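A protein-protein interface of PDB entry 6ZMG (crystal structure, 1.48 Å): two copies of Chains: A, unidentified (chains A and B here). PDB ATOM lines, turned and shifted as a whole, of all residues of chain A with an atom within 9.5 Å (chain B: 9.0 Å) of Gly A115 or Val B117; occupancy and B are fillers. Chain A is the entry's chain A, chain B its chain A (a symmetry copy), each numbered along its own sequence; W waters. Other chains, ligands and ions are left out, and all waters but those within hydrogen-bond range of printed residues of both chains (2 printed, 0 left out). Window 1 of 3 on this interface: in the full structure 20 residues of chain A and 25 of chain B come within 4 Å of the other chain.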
ATOM      1  N   LEU A   6     -29.209  27.808 -28.920  1.00  0.00           N
ATOM      2  CA  LEU A   6     -27.779  27.884 -28.685  1.00  0.00           C
ATOM      3  C   LEU A   6     -27.044  27.079 -29.740  1.00  0.00           C
ATOM      4  O   LEU A   6     -27.397  25.925 -30.020  1.00  0.00           O
ATOM      5  CB  LEU A   6     -27.426  27.353 -27.302  1.00  0.00           C
ATOM      6  CG  LEU A   6     -25.916  27.277 -27.045  1.00  0.00           C
ATOM      7  CD1 LEU A   6     -25.243  28.635 -27.268  1.00  0.00           C
ATOM      8  CD2 LEU A   6     -25.649  26.746 -25.627  1.00  0.00           C
ATOM      9  N   GLY A   8     -23.235  25.648 -31.536  1.00  0.00           N
ATOM     10  CA  GLY A   8     -22.088  24.870 -31.134  1.00  0.00           C
ATOM     11  C   GLY A   8     -22.403  23.393 -31.017  1.00  0.00           C
ATOM     12  O   GLY A   8     -23.472  22.896 -31.389  1.00  0.00           O
ATOM     13  N   GLY A   9     -21.419  22.679 -30.493  1.00  0.00           N
ATOM     14  CA  GLY A   9     -21.544  21.261 -30.285  1.00  0.00           C
ATOM     15  C   GLY A   9     -22.240  20.880 -29.006  1.00  0.00           C
ATOM     16  O   GLY A   9     -22.291  19.697 -28.664  1.00  0.00           O
ATOM     17  N   GLY A  10     -22.759  21.864 -28.284  1.00  0.00           N
ATOM     18  CA  GLY A  10     -23.498  21.578 -27.078  1.00  0.00           C
ATOM     19  C   GLY A  10     -22.647  21.082 -25.935  1.00  0.00           C
ATOM     20  O   GLY A  10     -23.019  20.107 -25.273  1.00  0.00           O
ATOM     21  N   PHE A  11     -21.514  21.721 -25.681  1.00  0.00           N
ATOM     22  CA  PHE A  11     -20.681  21.304 -24.565  1.00  0.00           C
ATOM     23  C   PHE A  11     -21.133  21.942 -23.261  1.00  0.00           C
ATOM     24  O   PHE A  11     -21.607  23.087 -23.217  1.00  0.00           O
ATOM     25  CB  PHE A  11     -19.216  21.632 -24.844  1.00  0.00           C
ATOM     26  CG  PHE A  11     -18.708  20.961 -26.062  1.00  0.00           C
ATOM     27  CD1 PHE A  11     -18.613  19.578 -26.102  1.00  0.00           C
ATOM     28  CD2 PHE A  11     -18.383  21.689 -27.192  1.00  0.00           C
ATOM     29  CE1 PHE A  11     -18.179  18.930 -27.240  1.00  0.00           C
ATOM     30  CE2 PHE A  11     -17.944  21.044 -28.336  1.00  0.00           C
ATOM     31  CZ  PHE A  11     -17.846  19.658 -28.356  1.00  0.00           C
ATOM     32  N   SER A  12     -20.970  21.168 -22.191  1.00  0.00           N
ATOM     33  CA  SER A  12     -21.193  21.638 -20.839  1.00  0.00           C
ATOM     34  C   SER A  12     -20.284  20.853 -19.910  1.00  0.00           C
ATOM     35  O   SER A  12     -19.683  19.843 -20.288  1.00  0.00           O
ATOM     36  CB  SER A  12     -22.654  21.470 -20.432  1.00  0.00           C
ATOM     37  OG  SER A  12     -23.035  20.102 -20.338  1.00  0.00           O
ATOM     38  N   ALA A  13     -20.174  21.345 -18.684  1.00  0.00           N
ATOM     39  CA  ALA A  13     -19.345  20.691 -17.698  1.00  0.00           C
ATOM     40  C   ALA A  13     -19.948  20.871 -16.318  1.00  0.00           C
ATOM     41  O   ALA A  13     -20.724  21.799 -16.058  1.00  0.00           O
ATOM     42  CB  ALA A  13     -17.932  21.282 -17.673  1.00  0.00           C
ATOM     43  N   ARG A  14     -19.558  19.955 -15.438  1.00  0.00           N
ATOM     44  CA  ARG A  14     -19.825  20.023 -14.012  1.00  0.00           C
ATOM     45  C   ARG A  14     -18.500  19.822 -13.291  1.00  0.00           C
ATOM     46  O   ARG A  14     -17.722  18.924 -13.643  1.00  0.00           O
ATOM     47  CB  ARG A  14     -20.800  18.927 -13.574  1.00  0.00           C
ATOM     48  CG  ARG A  14     -22.193  19.076 -14.077  1.00  0.00           C
ATOM     49  CD  ARG A  14     -23.139  18.336 -13.131  1.00  0.00           C
ATOM     50  NE  ARG A  14     -22.941  16.890 -13.155  1.00  0.00           N
ATOM     51  CZ  ARG A  14     -23.637  16.021 -12.424  1.00  0.00           C
ATOM     52  NH1 ARG A  14     -24.562  16.444 -11.565  1.00  0.00           N
ATOM     53  NH2 ARG A  14     -23.386  14.723 -12.533  1.00  0.00           N
ATOM     54  N   ILE A  77     -22.375  25.881 -18.952  1.00  0.00           N
ATOM     55  CA  ILE A  77     -22.893  25.644 -20.298  1.00  0.00           C
ATOM     56  C   ILE A  77     -22.086  26.516 -21.250  1.00  0.00           C
ATOM     57  O   ILE A  77     -21.979  27.731 -21.044  1.00  0.00           O
ATOM     58  CB  ILE A  77     -24.393  25.972 -20.391  1.00  0.00           C
ATOM     59  CG1 ILE A  77     -25.187  25.135 -19.387  1.00  0.00           C
ATOM     60  CG2 ILE A  77     -24.911  25.748 -21.819  1.00  0.00           C
ATOM     61  CD1 ILE A  77     -26.595  25.560 -19.237  1.00  0.00           C
ATOM     62  N   GLU A 110     -16.710  16.650 -14.932  1.00  0.00           N
ATOM     63  CA  GLU A 110     -17.503  15.893 -15.895  1.00  0.00           C
ATOM     64  C   GLU A 110     -17.769  16.775 -17.108  1.00  0.00           C
ATOM     65  O   GLU A 110     -18.300  17.883 -16.966  1.00  0.00           O
ATOM     66  CB  GLU A 110     -18.826  15.434 -15.263  1.00  0.00           C
ATOM     67  CG  GLU A 110     -19.710  14.623 -16.199  1.00  0.00           C
ATOM     68  CD  GLU A 110     -21.070  14.283 -15.624  1.00  0.00           C
ATOM     69  OE1 GLU A 110     -21.212  13.210 -15.014  1.00  0.00           O
ATOM     70  OE2 GLU A 110     -22.011  15.076 -15.797  1.00  0.00           O
ATOM     71  N   ILE A 111     -17.398  16.280 -18.292  1.00  0.00           N
ATOM     72  CA  ILE A 111     -17.590  16.970 -19.557  1.00  0.00           C
ATOM     73  C   ILE A 111     -18.729  16.275 -20.282  1.00  0.00           C
ATOM     74  O   ILE A 111     -18.708  15.046 -20.430  1.00  0.00           O
ATOM     75  CB  ILE A 111     -16.340  16.893 -20.454  1.00  0.00           C
ATOM     76  CG1 ILE A 111     -15.098  17.417 -19.747  1.00  0.00           C
ATOM     77  CG2 ILE A 111     -16.602  17.635 -21.755  1.00  0.00           C
ATOM     78  CD1 ILE A 111     -15.146  18.864 -19.427  1.00  0.00           C
ATOM     79  N   GLN A 112     -19.684  17.056 -20.781  1.00  0.00           N
ATOM     80  CA  GLN A 112     -20.810  16.531 -21.532  1.00  0.00           C
ATOM     81  C   GLN A 112     -20.897  17.191 -22.898  1.00  0.00           C
ATOM     82  O   GLN A 112     -20.488  18.344 -23.081  1.00  0.00           O
ATOM     83  CB  GLN A 112     -22.134  16.786 -20.802  1.00  0.00           C
ATOM     84  CG  GLN A 112     -22.235  16.029 -19.487  1.00  0.00           C
ATOM     85  CD  GLN A 112     -23.511  16.310 -18.755  1.00  0.00           C
ATOM     86  OE1 GLN A 112     -24.413  16.951 -19.289  1.00  0.00           O
ATOM     87  NE2 GLN A 112     -23.602  15.836 -17.520  1.00  0.00           N
ATOM     88  N   GLU A 113     -21.426  16.431 -23.854  1.00  0.00           N
ATOM     89  CA  GLU A 113     -21.728  16.909 -25.201  1.00  0.00           C
ATOM     90  C   GLU A 113     -23.181  16.530 -25.463  1.00  0.00           C
ATOM     91  O   GLU A 113     -23.515  15.343 -25.532  1.00  0.00           O
ATOM     92  CB  GLU A 113     -20.792  16.284 -26.238  1.00  0.00           C
ATOM     93  CG  GLU A 113     -21.034  16.775 -27.672  1.00  0.00           C
ATOM     94  CD  GLU A 113     -19.983  16.298 -28.656  1.00  0.00           C
ATOM     95  OE1 GLU A 113     -19.084  15.528 -28.244  1.00  0.00           O
ATOM     96  OE2 GLU A 113     -20.057  16.698 -29.841  1.00  0.00           O
ATOM     97  N   ARG A 114     -24.049  17.534 -25.584  1.00  0.00           N
ATOM     98  CA  ARG A 114     -25.497  17.326 -25.661  1.00  0.00           C
ATOM     99  C   ARG A 114     -25.996  16.455 -24.515  1.00  0.00           C
ATOM    100  O   ARG A 114     -26.881  15.608 -24.678  1.00  0.00           O
ATOM    101  CB  ARG A 114     -25.904  16.748 -27.008  1.00  0.00           C
ATOM    102  CG  ARG A 114     -25.467  17.615 -28.162  1.00  0.00           C
ATOM    103  CD  ARG A 114     -26.005  17.096 -29.477  1.00  0.00           C
ATOM    104  NE  ARG A 114     -25.125  16.067 -30.024  1.00  0.00           N
ATOM    105  CZ  ARG A 114     -23.932  16.315 -30.561  1.00  0.00           C
ATOM    106  NH1 ARG A 114     -23.470  17.561 -30.623  1.00  0.00           N
ATOM    107  NH2 ARG A 114     -23.194  15.316 -31.030  1.00  0.00           N
ATOM    108  N   GLY A 115     -25.400  16.643 -23.343  1.00  0.00           N
ATOM    109  CA  GLY A 115     -25.791  15.905 -22.168  1.00  0.00           C
ATOM    110  C   GLY A 115     -25.162  14.543 -22.023  1.00  0.00           C
ATOM    111  O   GLY A 115     -25.264  13.952 -20.945  1.00  0.00           O
ATOM    112  N   ILE A 116     -24.510  14.031 -23.058  1.00  0.00           N
ATOM    113  CA  ILE A 116     -23.858  12.732 -23.000  1.00  0.00           C
ATOM    114  C   ILE A 116     -22.460  12.917 -22.436  1.00  0.00           C
ATOM    115  O   ILE A 116     -21.689  13.763 -22.910  1.00  0.00           O
ATOM    116  CB  ILE A 116     -23.831  12.072 -24.390  1.00  0.00           C
ATOM    117  CG1 ILE A 116     -25.270  11.977 -24.915  1.00  0.00           C
ATOM    118  CG2 ILE A 116     -23.131  10.730 -24.291  1.00  0.00           C
ATOM    119  CD1 ILE A 116     -25.394  11.389 -26.291  1.00  0.00           C
ATOM    120  N   VAL A 117     -22.136  12.137 -21.410  1.00  0.00           N
ATOM    121  CA  VAL A 117     -20.869  12.310 -20.717  1.00  0.00           C
ATOM    122  C   VAL A 117     -19.744  11.822 -21.615  1.00  0.00           C
ATOM    123  O   VAL A 117     -19.709  10.650 -22.012  1.00  0.00           O
ATOM    124  CB  VAL A 117     -20.869  11.565 -19.381  1.00  0.00           C
ATOM    125  CG1 VAL A 117     -19.506  11.647 -18.716  1.00  0.00           C
ATOM    126  CG2 VAL A 117     -21.928  12.152 -18.473  1.00  0.00           C
ATOM    127  N   GLN A 118     -18.798  12.716 -21.898  1.00  0.00           N
ATOM    128  CA  GLN A 118     -17.620  12.393 -22.686  1.00  0.00           C
ATOM    129  C   GLN A 118     -16.495  11.870 -21.815  1.00  0.00           C
ATOM    130  O   GLN A 118     -15.744  10.981 -22.230  1.00  0.00           O
ATOM    131  CB  GLN A 118     -17.158  13.640 -23.436  1.00  0.00           C
ATOM    132  CG  GLN A 118     -18.231  14.208 -24.323  1.00  0.00           C
ATOM    133  CD  GLN A 118     -18.708  13.200 -25.337  1.00  0.00           C
ATOM    134  OE1 GLN A 118     -17.937  12.773 -26.200  1.00  0.00           O
ATOM    135  NE2 GLN A 118     -19.976  12.795 -25.235  1.00  0.00           N
ATOM    136  N   ASP A 119     -16.357  12.434 -20.620  1.00  0.00           N
ATOM    137  CA  ASP A 119     -15.271  12.097 -19.723  1.00  0.00           C
ATOM    138  C   ASP A 119     -15.715  12.490 -18.319  1.00  0.00           C
ATOM    139  O   ASP A 119     -16.361  13.524 -18.146  1.00  0.00           O
ATOM    140  CB  ASP A 119     -13.989  12.899 -20.029  1.00  0.00           C
ATOM    141  CG  ASP A 119     -13.739  13.132 -21.532  1.00  0.00           C
ATOM    142  OD1 ASP A 119     -13.235  12.201 -22.208  1.00  0.00           O
ATOM    143  OD2 ASP A 119     -14.011  14.259 -22.027  1.00  0.00           O
ATOM    144  N   GLY B  10     -39.537  10.210 -21.946  1.00  0.00           N
ATOM    145  CA  GLY B  10     -38.474  10.609 -21.055  1.00  0.00           C
ATOM    146  C   GLY B  10     -38.060  12.053 -21.194  1.00  0.00           C
ATOM    147  O   GLY B  10     -36.860  12.344 -21.239  1.00  0.00           O
ATOM    148  N   SER B  12     -37.480  15.926 -19.969  1.00  0.00           N
ATOM    149  CA  SER B  12     -37.200  16.735 -18.800  1.00  0.00           C
ATOM    150  C   SER B  12     -36.675  18.080 -19.272  1.00  0.00           C
ATOM    151  O   SER B  12     -36.340  18.273 -20.444  1.00  0.00           O
ATOM    152  CB  SER B  12     -36.187  16.051 -17.887  1.00  0.00           C
ATOM    153  OG  SER B  12     -34.901  15.945 -18.490  1.00  0.00           O
ATOM    154  N   ALA B  13     -36.627  19.022 -18.340  1.00  0.00           N
ATOM    155  CA  ALA B  13     -36.142  20.346 -18.653  1.00  0.00           C
ATOM    156  C   ALA B  13     -35.438  20.935 -17.446  1.00  0.00           C
ATOM    157  O   ALA B  13     -35.671  20.542 -16.296  1.00  0.00           O
ATOM    158  CB  ALA B  13     -37.289  21.288 -19.034  1.00  0.00           C
ATOM    159  N   ARG B  14     -34.576  21.900 -17.746  1.00  0.00           N
ATOM    160  CA  ARG B  14     -33.933  22.758 -16.765  1.00  0.00           C
ATOM    161  C   ARG B  14     -34.148  24.197 -17.210  1.00  0.00           C
ATOM    162  O   ARG B  14     -33.977  24.523 -18.393  1.00  0.00           O
ATOM    163  CB  ARG B  14     -32.429  22.483 -16.683  1.00  0.00           C
ATOM    164  CG  ARG B  14     -32.054  21.161 -16.113  1.00  0.00           C
ATOM    165  CD  ARG B  14     -30.640  21.256 -15.540  1.00  0.00           C
ATOM    166  NE  ARG B  14     -29.627  21.461 -16.571  1.00  0.00           N
ATOM    167  CZ  ARG B  14     -28.322  21.577 -16.335  1.00  0.00           C
ATOM    168  NH1 ARG B  14     -27.853  21.551 -15.089  1.00  0.00           N
ATOM    169  NH2 ARG B  14     -27.484  21.746 -17.349  1.00  0.00           N
ATOM    170  N   LYS B  84     -43.371  15.223 -27.286  1.00  0.00           N
ATOM    171  CA  LYS B  84     -42.251  16.152 -27.382  1.00  0.00           C
ATOM    172  C   LYS B  84     -42.738  17.577 -27.625  1.00  0.00           C
ATOM    173  O   LYS B  84     -42.294  18.519 -26.959  1.00  0.00           O
ATOM    174  CB  LYS B  84     -41.319  15.714 -28.510  1.00  0.00           C
ATOM    175  CG  LYS B  84     -40.016  16.484 -28.567  1.00  0.00           C
ATOM    176  CD  LYS B  84     -39.063  15.830 -29.558  1.00  0.00           C
ATOM    177  CE  LYS B  84     -37.619  16.276 -29.345  1.00  0.00           C
ATOM    178  NZ  LYS B  84     -36.703  15.651 -30.364  1.00  0.00           N
ATOM    179  N   VAL B 109     -33.169  27.895 -21.033  1.00  0.00           N
ATOM    180  CA  VAL B 109     -34.003  26.703 -21.013  1.00  0.00           C
ATOM    181  C   VAL B 109     -33.268  25.576 -21.723  1.00  0.00           C
ATOM    182  O   VAL B 109     -32.762  25.759 -22.838  1.00  0.00           O
ATOM    183  CB  VAL B 109     -35.357  26.952 -21.703  1.00  0.00           C
ATOM    184  CG1 VAL B 109     -36.150  25.655 -21.817  1.00  0.00           C
ATOM    185  CG2 VAL B 109     -36.171  27.996 -20.962  1.00  0.00           C
ATOM    186  N   GLU B 110     -33.226  24.405 -21.091  1.00  0.00           N
ATOM    187  CA  GLU B 110     -32.627  23.208 -21.673  1.00  0.00           C
ATOM    188  C   GLU B 110     -33.657  22.087 -21.647  1.00  0.00           C
ATOM    189  O   GLU B 110     -34.196  21.762 -20.583  1.00  0.00           O
ATOM    190  CB  GLU B 110     -31.367  22.801 -20.893  1.00  0.00           C
ATOM    191  CG  GLU B 110     -30.671  21.565 -21.444  1.00  0.00           C
ATOM    192  CD  GLU B 110     -29.508  21.083 -20.601  1.00  0.00           C
ATOM    193  OE1 GLU B 110     -28.366  21.499 -20.860  1.00  0.00           O
ATOM    194  OE2 GLU B 110     -29.726  20.270 -19.687  1.00  0.00           O
ATOM    195  N   ILE B 111     -33.925  21.502 -22.819  1.00  0.00           N
ATOM    196  CA  ILE B 111     -34.863  20.404 -22.983  1.00  0.00           C
ATOM    197  C   ILE B 111     -34.046  19.143 -23.205  1.00  0.00           C
ATOM    198  O   ILE B 111     -33.164  19.123 -24.073  1.00  0.00           O
ATOM    199  CB  ILE B 111     -35.775  20.600 -24.208  1.00  0.00           C
ATOM    200  CG1 ILE B 111     -36.517  21.929 -24.158  1.00  0.00           C
ATOM    201  CG2 ILE B 111     -36.733  19.426 -24.322  1.00  0.00           C
ATOM    202  CD1 ILE B 111     -37.487  22.043 -23.043  1.00  0.00           C
ATOM    203  N   GLN B 112     -34.376  18.082 -22.473  1.00  0.00           N
ATOM    204  CA  GLN B 112     -33.709  16.800 -22.609  1.00  0.00           C
ATOM    205  C   GLN B 112     -34.715  15.701 -22.906  1.00  0.00           C
ATOM    206  O   GLN B 112     -35.882  15.774 -22.503  1.00  0.00           O
ATOM    207  CB  GLN B 112     -32.962  16.420 -21.325  1.00  0.00           C
ATOM    208  CG  GLN B 112     -31.807  17.359 -21.016  1.00  0.00           C
ATOM    209  CD  GLN B 112     -31.105  17.012 -19.740  1.00  0.00           C
ATOM    210  OE1 GLN B 112     -31.366  15.970 -19.144  1.00  0.00           O
ATOM    211  NE2 GLN B 112     -30.206  17.882 -19.303  1.00  0.00           N
ATOM    212  N   GLU B 113     -34.242  14.688 -23.629  1.00  0.00           N
ATOM    213  CA  GLU B 113     -34.994  13.468 -23.913  1.00  0.00           C
ATOM    214  C   GLU B 113     -34.085  12.313 -23.509  1.00  0.00           C
ATOM    215  O   GLU B 113     -33.028  12.109 -24.114  1.00  0.00           O
ATOM    216  CB  GLU B 113     -35.383  13.383 -25.390  1.00  0.00           C
ATOM    217  CG  GLU B 113     -36.209  12.140 -25.747  1.00  0.00           C
ATOM    218  CD  GLU B 113     -36.747  12.162 -27.165  1.00  0.00           C
ATOM    219  OE1 GLU B 113     -36.433  13.121 -27.908  1.00  0.00           O
ATOM    220  OE2 GLU B 113     -37.488  11.220 -27.532  1.00  0.00           O
ATOM    221  N   ARG B 114     -34.481  11.575 -22.472  1.00  0.00           N
ATOM    222  CA  ARG B 114     -33.634  10.548 -21.861  1.00  0.00           C
ATOM    223  C   ARG B 114     -32.260  11.101 -21.502  1.00  0.00           C
ATOM    224  O   ARG B 114     -31.231  10.433 -21.645  1.00  0.00           O
ATOM    225  CB  ARG B 114     -33.516   9.321 -22.753  1.00  0.00           C
ATOM    226  CG  ARG B 114     -34.858   8.721 -23.085  1.00  0.00           C
ATOM    227  CD  ARG B 114     -34.709   7.424 -23.851  1.00  0.00           C
ATOM    228  NE  ARG B 114     -34.564   7.685 -25.280  1.00  0.00           N
ATOM    229  CZ  ARG B 114     -35.558   8.086 -26.070  1.00  0.00           C
ATOM    230  NH1 ARG B 114     -36.776   8.279 -25.570  1.00  0.00           N
ATOM    231  NH2 ARG B 114     -35.335   8.305 -27.361  1.00  0.00           N
ATOM    232  N   GLY B 115     -32.238  12.351 -21.055  1.00  0.00           N
ATOM    233  CA  GLY B 115     -31.010  12.991 -20.655  1.00  0.00           C
ATOM    234  C   GLY B 115     -30.210  13.607 -21.774  1.00  0.00           C
ATOM    235  O   GLY B 115     -29.276  14.363 -21.491  1.00  0.00           O
ATOM    236  N   ILE B 116     -30.544  13.324 -23.025  1.00  0.00           N
ATOM    237  CA  ILE B 116     -29.838  13.888 -24.165  1.00  0.00           C
ATOM    238  C   ILE B 116     -30.450  15.238 -24.493  1.00  0.00           C
ATOM    239  O   ILE B 116     -31.673  15.363 -24.642  1.00  0.00           O
ATOM    240  CB  ILE B 116     -29.888  12.929 -25.367  1.00  0.00           C
ATOM    241  CG1 ILE B 116     -29.310  11.574 -24.938  1.00  0.00           C
ATOM    242  CG2 ILE B 116     -29.157  13.559 -26.538  1.00  0.00           C
ATOM    243  CD1 ILE B 116     -29.336  10.519 -26.007  1.00  0.00           C
ATOM    244  N   VAL B 117     -29.602  16.257 -24.590  1.00  0.00           N
ATOM    245  CA  VAL B 117     -30.090  17.613 -24.784  1.00  0.00           C
ATOM    246  C   VAL B 117     -30.623  17.750 -26.200  1.00  0.00           C
ATOM    247  O   VAL B 117     -29.889  17.554 -27.178  1.00  0.00           O
ATOM    248  CB  VAL B 117     -28.985  18.636 -24.510  1.00  0.00           C
ATOM    249  CG1 VAL B 117     -29.462  20.043 -24.828  1.00  0.00           C
ATOM    250  CG2 VAL B 117     -28.558  18.546 -23.062  1.00  0.00           C
ATOM    251  N   GLN B 118     -31.894  18.130 -26.308  1.00  0.00           N
ATOM    252  CA  GLN B 118     -32.538  18.373 -27.588  1.00  0.00           C
ATOM    253  C   GLN B 118     -32.347  19.806 -28.044  1.00  0.00           C
ATOM    254  O   GLN B 118     -32.193  20.066 -29.242  1.00  0.00           O
ATOM    255  CB  GLN B 118     -34.028  18.061 -27.470  1.00  0.00           C
ATOM    256  CG  GLN B 118     -34.286  16.649 -27.023  1.00  0.00           C
ATOM    257  CD  GLN B 118     -33.670  15.645 -27.963  1.00  0.00           C
ATOM    258  OE1 GLN B 118     -34.061  15.563 -29.130  1.00  0.00           O
ATOM    259  NE2 GLN B 118     -32.689  14.884 -27.474  1.00  0.00           N
ATOM    260  N   ASP B 119     -32.379  20.740 -27.100  1.00  0.00           N
ATOM    261  CA  ASP B 119     -32.302  22.153 -27.402  1.00  0.00           C
ATOM    262  C   ASP B 119     -31.833  22.856 -26.134  1.00  0.00           C
ATOM    263  O   ASP B 119     -32.246  22.480 -25.036  1.00  0.00           O
ATOM    264  CB  ASP B 119     -33.678  22.751 -27.763  1.00  0.00           C
ATOM    265  CG  ASP B 119     -34.575  21.806 -28.587  1.00  0.00           C
ATOM    266  OD1 ASP B 119     -34.371  21.711 -29.822  1.00  0.00           O
ATOM    267  OD2 ASP B 119     -35.509  21.191 -28.005  1.00  0.00           O
ATOM    268  N   VAL B 120     -30.965  23.851 -26.288  1.00  0.00           N
ATOM    269  CA  VAL B 120     -30.723  24.867 -25.272  1.00  0.00           C
ATOM    270  C   VAL B 120     -31.113  26.195 -25.901  1.00  0.00           C
ATOM    271  O   VAL B 120     -30.669  26.509 -27.015  1.00  0.00           O
ATOM    272  CB  VAL B 120     -29.250  24.946 -24.839  1.00  0.00           C
ATOM    273  CG1 VAL B 120     -29.067  26.054 -23.796  1.00  0.00           C
ATOM    274  CG2 VAL B 120     -28.756  23.652 -24.330  1.00  0.00           C
ATOM    275  N   TYR B 121     -31.958  26.952 -25.206  1.00  0.00           N
ATOM    276  CA  TYR B 121     -32.473  28.224 -25.676  1.00  0.00           C
ATOM    277  C   TYR B 121     -32.096  29.301 -24.672  1.00  0.00           C
ATOM    278  O   TYR B 121     -32.160  29.072 -23.459  1.00  0.00           O
ATOM    279  CB  TYR B 121     -34.030  28.246 -25.731  1.00  0.00           C
ATOM    280  CG  TYR B 121     -34.655  27.131 -26.499  1.00  0.00           C
ATOM    281  CD1 TYR B 121     -34.739  27.186 -27.879  1.00  0.00           C
ATOM    282  CD2 TYR B 121     -35.223  26.056 -25.850  1.00  0.00           C
ATOM    283  CE1 TYR B 121     -35.325  26.166 -28.603  1.00  0.00           C
ATOM    284  CE2 TYR B 121     -35.804  25.020 -26.560  1.00  0.00           C
ATOM    285  CZ  TYR B 121     -35.856  25.081 -27.941  1.00  0.00           C
ATOM    286  OH  TYR B 121     -36.446  24.071 -28.669  1.00  0.00           O
HETATM  287  O   HOH W   1     -27.544  14.000 -19.322  1.00  0.00           O
HETATM  288  O   HOH W   2     -29.085  24.016 -28.663  1.00  0.00           O
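N of Leu A6 sits at hydrogen-bond distance from O of Val B120 (2.7 Å).
O of Arg A114 lies within hydrogen-bond range of N of Val B117, 2.8 Å away.
O of Gly A9 is in hydrogen-bond range of NH1 of Arg A114 (3.1 Å).
O of Gly A10 is in hydrogen-bond range of N of Arg A114 (2.8 Å).
The side-chain carboxylate (OE2) of Glu A113 is in salt-bridge range of the guanidinium group (NH1) of Arg A114, at 3.6 Å.
O of Ile B116 sits at hydrogen-bond distance from NE2 of Gln B118, 3.0 Å away.
Arg A114 touches Ile B116 (O to CA, 3.5 Å).
CA of Gly A115 touches O of Gly B115, at 3.9 Å.
Gly A115 touches Val B117.
Of the printed residues of chain B, Leu A6 touches Val B120.
Of the printed residues of chain B, Arg A114 touches Ile B116 (3.5 Å) and Val B117 (2.8 Å).
Of chain B, only Gly B115 and Val B117 come within 4 Å of Gly A115.
Gly B10 touches none of the printed residues of chain A.
Printed residues of chain A within 4 Å of Ile B116: Arg A114.
Val B117 touches just these residues of chain A: Arg A114 (2.8 Å) and Gly A115 (3.7 Å).
No residue of chain A comes within 4 Å of Gln B118.
The nearest residue of chain B that does not touch Gly A115 is Ile B116 (4.9 Å).
Of the 19 printed residues of chain A, 3 touch a printed residue of chain B.
Hydrophobic or aromatic side chains of chain A within 4 Å of the printed part of chain B: Leu A6.
Arg A114 touches Ile B116, but with the chains exchanged Ile A116 does not touch Arg B114 (7.0 Å).
Arg A114 touches Val B117, but with the chains exchanged Val A117 does not touch Arg B114 (9.3 Å).
Gly B115 touches its own counterpart, Gly A115.
Gly A115 touches Val B117, but with the chains exchanged Val A117 does not touch Gly B115 (7.5 Å).
Of the 5 pairs that touch across the chains among the printed residues, 1 has its exchanged pair printed and touching as well.
Water W1 bridges the backbone carbonyl oxygen of Gly A115 (2.8 Å) and the backbone carbonyl oxygen of Gly B115 (2.8 Å).
Water W2 lies within hydrogen-bond range of O of Leu A6 (2.9 Å) and N of Val B120 (3.0 Å).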
